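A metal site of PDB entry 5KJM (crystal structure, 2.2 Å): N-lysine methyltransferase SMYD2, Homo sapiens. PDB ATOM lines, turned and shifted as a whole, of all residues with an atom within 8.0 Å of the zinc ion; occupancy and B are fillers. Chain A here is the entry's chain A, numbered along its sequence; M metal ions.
SG of Cys 86 lies close to NH1 of Arg 63 (3.8 Å). The side-chain sulfur (SG) of Cys 64 lies close to the backbone NH (N) of Gln 66 (3.5 Å). N of Cys 61 lies within hydrogen-bond range of O of Ala 67 (2.8 Å). The side-chain sulfur (SG) of Cys 61 sits close to the backbone NH (N) of Arg 63, at 3.6 Å.
Four residues have an atom within 4 Å of the zinc ion: Cys 61, Cys 64, His 82 and Cys 86. The nearest printed residue that does not touch the zinc ion is Arg 63 (4.4 Å).
The zinc ion is bound by SG of Cys 64 (2.2 Å). The zinc ion is bound by a ring nitrogen (NE2) of His 82. The zinc ion is bound by SG of Cys 86, 2.4 Å away. SG of Cys 61 is bound to the zinc ion (2.4 Å). The zinc ion has four donor atoms within binding distance.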
ATOM      1  N   LYS A  60       5.942  -5.134  -5.704  1.00  0.00           N
ATOM      2  CA  LYS A  60       6.822  -5.999  -4.926  1.00  0.00           C
ATOM      3  C   LYS A  60       6.847  -7.408  -5.548  1.00  0.00           C
ATOM      4  O   LYS A  60       5.782  -7.899  -5.927  1.00  0.00           O
ATOM      5  CB  LYS A  60       6.246  -6.088  -3.500  1.00  0.00           C
ATOM      6  CG  LYS A  60       7.141  -6.696  -2.440  1.00  0.00           C
ATOM      7  CD  LYS A  60       6.334  -6.985  -1.173  1.00  0.00           C
ATOM      8  CE  LYS A  60       6.512  -5.944  -0.082  1.00  0.00           C
ATOM      9  NZ  LYS A  60       5.807  -6.327   1.167  1.00  0.00           N
ATOM     10  N   CYS A  61       8.049  -8.068  -5.619  1.00  0.00           N
ATOM     11  CA  CYS A  61       8.128  -9.456  -6.109  1.00  0.00           C
ATOM     12  C   CYS A  61       7.467 -10.320  -5.032  1.00  0.00           C
ATOM     13  O   CYS A  61       7.896 -10.297  -3.880  1.00  0.00           O
ATOM     14  CB  CYS A  61       9.551  -9.913  -6.398  1.00  0.00           C
ATOM     15  SG  CYS A  61       9.694 -11.700  -6.710  1.00  0.00           S
ATOM     16  N   GLY A  62       6.403 -11.019  -5.406  1.00  0.00           N
ATOM     17  CA  GLY A  62       5.611 -11.835  -4.503  1.00  0.00           C
ATOM     18  C   GLY A  62       6.355 -12.987  -3.849  1.00  0.00           C
ATOM     19  O   GLY A  62       5.974 -13.414  -2.757  1.00  0.00           O
ATOM     20  N   ARG A  63       7.399 -13.491  -4.520  1.00  0.00           N
ATOM     21  CA  ARG A  63       8.180 -14.628  -4.048  1.00  0.00           C
ATOM     22  C   ARG A  63       9.128 -14.254  -2.919  1.00  0.00           C
ATOM     23  O   ARG A  63       9.043 -14.836  -1.836  1.00  0.00           O
ATOM     24  CB  ARG A  63       8.908 -15.287  -5.221  1.00  0.00           C
ATOM     25  CG  ARG A  63       9.122 -16.784  -5.024  1.00  0.00           C
ATOM     26  CD  ARG A  63      10.006 -17.381  -6.108  1.00  0.00           C
ATOM     27  NE  ARG A  63       9.247 -17.805  -7.283  1.00  0.00           N
ATOM     28  CZ  ARG A  63       9.125 -17.091  -8.397  1.00  0.00           C
ATOM     29  NH1 ARG A  63       9.724 -15.902  -8.495  1.00  0.00           N
ATOM     30  NH2 ARG A  63       8.423 -17.551  -9.412  1.00  0.00           N
ATOM     31  N   CYS A  64      10.033 -13.288  -3.166  1.00  0.00           N
ATOM     32  CA  CYS A  64      11.053 -12.849  -2.206  1.00  0.00           C
ATOM     33  C   CYS A  64      10.625 -11.636  -1.365  1.00  0.00           C
ATOM     34  O   CYS A  64      11.135 -11.469  -0.264  1.00  0.00           O
ATOM     35  CB  CYS A  64      12.379 -12.589  -2.917  1.00  0.00           C
ATOM     36  SG  CYS A  64      12.338 -11.193  -4.083  1.00  0.00           S
ATOM     37  N   LYS A  65       9.754 -10.763  -1.922  1.00  0.00           N
ATOM     38  CA  LYS A  65       9.258  -9.518  -1.281  1.00  0.00           C
ATOM     39  C   LYS A  65      10.402  -8.497  -1.068  1.00  0.00           C
ATOM     40  O   LYS A  65      10.284  -7.570  -0.269  1.00  0.00           O
ATOM     41  CB  LYS A  65       8.474  -9.806   0.021  1.00  0.00           C
ATOM     42  CG  LYS A  65       7.222 -10.653  -0.200  1.00  0.00           C
ATOM     43  CD  LYS A  65       6.721 -11.257   1.110  1.00  0.00           C
ATOM     44  CE  LYS A  65       5.481 -12.101   0.897  1.00  0.00           C
ATOM     45  NZ  LYS A  65       5.796 -13.384   0.225  1.00  0.00           N
ATOM     46  N   GLN A  66      11.507  -8.677  -1.820  1.00  0.00           N
ATOM     47  CA  GLN A  66      12.703  -7.866  -1.690  1.00  0.00           C
ATOM     48  C   GLN A  66      13.263  -7.385  -3.044  1.00  0.00           C
ATOM     49  O   GLN A  66      14.470  -7.143  -3.184  1.00  0.00           O
ATOM     50  CB  GLN A  66      13.756  -8.597  -0.850  1.00  0.00           C
ATOM     51  CG  GLN A  66      13.398  -8.694   0.629  1.00  0.00           C
ATOM     52  CD  GLN A  66      14.410  -9.509   1.368  1.00  0.00           C
ATOM     53  OE1 GLN A  66      15.429  -9.001   1.850  1.00  0.00           O
ATOM     54  NE2 GLN A  66      14.165 -10.803   1.473  1.00  0.00           N
ATOM     55  N   ALA A  67      12.361  -7.225  -4.026  1.00  0.00           N
ATOM     56  CA  ALA A  67      12.625  -6.716  -5.368  1.00  0.00           C
ATOM     57  C   ALA A  67      11.400  -5.904  -5.787  1.00  0.00           C
ATOM     58  O   ALA A  67      10.268  -6.374  -5.607  1.00  0.00           O
ATOM     59  CB  ALA A  67      12.866  -7.860  -6.341  1.00  0.00           C
ATOM     60  N   PHE A  68      11.600  -4.664  -6.229  1.00  0.00           N
ATOM     61  CA  PHE A  68      10.480  -3.793  -6.584  1.00  0.00           C
ATOM     62  C   PHE A  68      10.588  -3.338  -8.037  1.00  0.00           C
ATOM     63  O   PHE A  68      11.690  -3.073  -8.534  1.00  0.00           O
ATOM     64  CB  PHE A  68      10.307  -2.618  -5.585  1.00  0.00           C
ATOM     65  CG  PHE A  68      10.019  -3.043  -4.163  1.00  0.00           C
ATOM     66  CD1 PHE A  68       8.733  -2.944  -3.640  1.00  0.00           C
ATOM     67  CD2 PHE A  68      11.022  -3.554  -3.339  1.00  0.00           C
ATOM     68  CE1 PHE A  68       8.462  -3.330  -2.316  1.00  0.00           C
ATOM     69  CE2 PHE A  68      10.755  -3.938  -2.025  1.00  0.00           C
ATOM     70  CZ  PHE A  68       9.486  -3.826  -1.525  1.00  0.00           C
ATOM     71  N   TYR A  69       9.434  -3.323  -8.739  1.00  0.00           N
ATOM     72  CA  TYR A  69       9.346  -3.045 -10.171  1.00  0.00           C
ATOM     73  C   TYR A  69       8.269  -2.034 -10.552  1.00  0.00           C
ATOM     74  O   TYR A  69       7.259  -1.921  -9.851  1.00  0.00           O
ATOM     75  CB  TYR A  69       9.110  -4.365 -10.925  1.00  0.00           C
ATOM     76  CG  TYR A  69      10.184  -5.403 -10.686  1.00  0.00           C
ATOM     77  CD1 TYR A  69      10.012  -6.406  -9.730  1.00  0.00           C
ATOM     78  CD2 TYR A  69      11.388  -5.362 -11.377  1.00  0.00           C
ATOM     79  CE1 TYR A  69      11.002  -7.368  -9.511  1.00  0.00           C
ATOM     80  CE2 TYR A  69      12.361  -6.338 -11.192  1.00  0.00           C
ATOM     81  CZ  TYR A  69      12.176  -7.323 -10.240  1.00  0.00           C
ATOM     82  OH  TYR A  69      13.175  -8.253 -10.056  1.00  0.00           O
ATOM     83  N   GLN A  75       9.500  -6.428 -14.220  1.00  0.00           N
ATOM     84  CA  GLN A  75       9.647  -7.649 -13.439  1.00  0.00           C
ATOM     85  C   GLN A  75      10.140  -8.840 -14.289  1.00  0.00           C
ATOM     86  O   GLN A  75      11.136  -9.461 -13.915  1.00  0.00           O
ATOM     87  CB  GLN A  75       8.356  -7.970 -12.663  1.00  0.00           C
ATOM     88  CG  GLN A  75       8.509  -9.163 -11.716  1.00  0.00           C
ATOM     89  CD  GLN A  75       7.332  -9.428 -10.816  1.00  0.00           C
ATOM     90  OE1 GLN A  75       7.347 -10.373 -10.017  1.00  0.00           O
ATOM     91  NE2 GLN A  75       6.286  -8.616 -10.904  1.00  0.00           N
ATOM     92  N   ASP A  78      13.749  -8.351 -15.690  1.00  0.00           N
ATOM     93  CA  ASP A  78      14.788  -8.487 -14.680  1.00  0.00           C
ATOM     94  C   ASP A  78      14.983  -9.908 -14.164  1.00  0.00           C
ATOM     95  O   ASP A  78      16.028 -10.186 -13.590  1.00  0.00           O
ATOM     96  CB  ASP A  78      14.570  -7.516 -13.506  1.00  0.00           C
ATOM     97  CG  ASP A  78      15.764  -7.356 -12.577  1.00  0.00           C
ATOM     98  OD1 ASP A  78      15.642  -7.702 -11.376  1.00  0.00           O
ATOM     99  OD2 ASP A  78      16.853  -6.938 -13.069  1.00  0.00           O
ATOM    100  N   TRP A  79      14.016 -10.810 -14.405  1.00  0.00           N
ATOM    101  CA  TRP A  79      14.029 -12.203 -13.944  1.00  0.00           C
ATOM    102  C   TRP A  79      15.314 -12.977 -14.305  1.00  0.00           C
ATOM    103  O   TRP A  79      15.868 -13.574 -13.383  1.00  0.00           O
ATOM    104  CB  TRP A  79      12.765 -13.000 -14.355  1.00  0.00           C
ATOM    105  CG  TRP A  79      12.750 -14.408 -13.820  1.00  0.00           C
ATOM    106  CD1 TRP A  79      12.815 -15.553 -14.554  1.00  0.00           C
ATOM    107  CD2 TRP A  79      12.743 -14.808 -12.444  1.00  0.00           C
ATOM    108  NE1 TRP A  79      12.836 -16.651 -13.717  1.00  0.00           N
ATOM    109  CE2 TRP A  79      12.795 -16.222 -12.418  1.00  0.00           C
ATOM    110  CE3 TRP A  79      12.735 -14.117 -11.214  1.00  0.00           C
ATOM    111  CZ2 TRP A  79      12.783 -16.956 -11.218  1.00  0.00           C
ATOM    112  CZ3 TRP A  79      12.743 -14.830 -10.034  1.00  0.00           C
ATOM    113  CH2 TRP A  79      12.752 -16.236 -10.041  1.00  0.00           C
ATOM    114  N   HIS A  82      17.417 -11.380 -11.569  1.00  0.00           N
ATOM    115  CA  HIS A  82      16.760 -11.529 -10.262  1.00  0.00           C
ATOM    116  C   HIS A  82      16.693 -12.984  -9.727  1.00  0.00           C
ATOM    117  O   HIS A  82      16.811 -13.198  -8.508  1.00  0.00           O
ATOM    118  CB  HIS A  82      15.366 -10.890 -10.259  1.00  0.00           C
ATOM    119  CG  HIS A  82      14.736 -10.917  -8.910  1.00  0.00           C
ATOM    120  ND1 HIS A  82      15.407 -10.449  -7.784  1.00  0.00           N
ATOM    121  CD2 HIS A  82      13.532 -11.406  -8.532  1.00  0.00           C
ATOM    122  CE1 HIS A  82      14.599 -10.671  -6.769  1.00  0.00           C
ATOM    123  NE2 HIS A  82      13.463 -11.231  -7.160  1.00  0.00           N
ATOM    124  N   LYS A  83      16.574 -13.964 -10.644  1.00  0.00           N
ATOM    125  CA  LYS A  83      16.534 -15.410 -10.388  1.00  0.00           C
ATOM    126  C   LYS A  83      17.763 -15.896  -9.546  1.00  0.00           C
ATOM    127  O   LYS A  83      17.631 -16.845  -8.755  1.00  0.00           O
ATOM    128  CB  LYS A  83      16.389 -16.140 -11.746  1.00  0.00           C
ATOM    129  CG  LYS A  83      16.818 -17.588 -11.839  1.00  0.00           C
ATOM    130  CD  LYS A  83      17.391 -17.872 -13.241  1.00  0.00           C
ATOM    131  CE  LYS A  83      16.418 -18.497 -14.215  1.00  0.00           C
ATOM    132  NZ  LYS A  83      16.040 -19.903 -13.865  1.00  0.00           N
ATOM    133  N   GLU A  85      19.088 -14.310  -7.018  1.00  0.00           N
ATOM    134  CA  GLU A  85      18.880 -13.846  -5.652  1.00  0.00           C
ATOM    135  C   GLU A  85      17.509 -14.116  -5.022  1.00  0.00           C
ATOM    136  O   GLU A  85      17.418 -14.197  -3.801  1.00  0.00           O
ATOM    137  CB  GLU A  85      19.188 -12.340  -5.593  1.00  0.00           C
ATOM    138  CG  GLU A  85      20.660 -12.035  -5.837  1.00  0.00           C
ATOM    139  CD  GLU A  85      21.072 -10.584  -5.778  1.00  0.00           C
ATOM    140  OE1 GLU A  85      20.202  -9.692  -5.912  1.00  0.00           O
ATOM    141  OE2 GLU A  85      22.287 -10.339  -5.619  1.00  0.00           O
ATOM    142  N   CYS A  86      16.439 -14.232  -5.836  1.00  0.00           N
ATOM    143  CA  CYS A  86      15.058 -14.412  -5.379  1.00  0.00           C
ATOM    144  C   CYS A  86      14.876 -15.527  -4.321  1.00  0.00           C
ATOM    145  O   CYS A  86      14.669 -15.216  -3.136  1.00  0.00           O
ATOM    146  CB  CYS A  86      14.112 -14.608  -6.560  1.00  0.00           C
ATOM    147  SG  CYS A  86      12.356 -14.533  -6.122  1.00  0.00           S
ATOM    148  N   SER A  87      14.923 -16.804  -4.732  1.00  0.00           N
ATOM    149  CA  SER A  87      14.829 -17.923  -3.799  1.00  0.00           C
ATOM    150  C   SER A  87      16.014 -17.891  -2.791  1.00  0.00           C
ATOM    151  O   SER A  87      15.733 -17.977  -1.588  1.00  0.00           O
ATOM    152  CB  SER A  87      14.756 -19.263  -4.529  1.00  0.00           C
ATOM    153  OG  SER A  87      14.540 -20.280  -3.576  1.00  0.00           O
ATOM    154  N   MET A  89      17.588 -15.494  -1.252  1.00  0.00           N
ATOM    155  CA  MET A  89      17.275 -14.520  -0.195  1.00  0.00           C
ATOM    156  C   MET A  89      16.336 -15.075   0.853  1.00  0.00           C
ATOM    157  O   MET A  89      16.515 -14.770   2.019  1.00  0.00           O
ATOM    158  CB  MET A  89      16.686 -13.210  -0.770  1.00  0.00           C
ATOM    159  CG  MET A  89      17.746 -12.197  -1.201  1.00  0.00           C
ATOM    160  SD  MET A  89      17.084 -10.574  -1.735  1.00  0.00           S
ATOM    161  CE  MET A  89      16.272 -11.026  -3.314  1.00  0.00           C
ATOM    162  N   VAL A  90      15.300 -15.833   0.450  1.00  0.00           N
ATOM    163  CA  VAL A  90      14.333 -16.355   1.408  1.00  0.00           C
ATOM    164  C   VAL A  90      14.893 -17.620   2.112  1.00  0.00           C
ATOM    165  O   VAL A  90      14.691 -17.776   3.322  1.00  0.00           O
ATOM    166  CB  VAL A  90      12.878 -16.504   0.846  1.00  0.00           C
ATOM    167  CG1 VAL A  90      12.820 -16.688  -0.671  1.00  0.00           C
ATOM    168  CG2 VAL A  90      12.040 -17.548   1.580  1.00  0.00           C
HETATM  169 ZN    ZN M   1      11.959 -12.216  -5.943  1.00  0.00          ZN
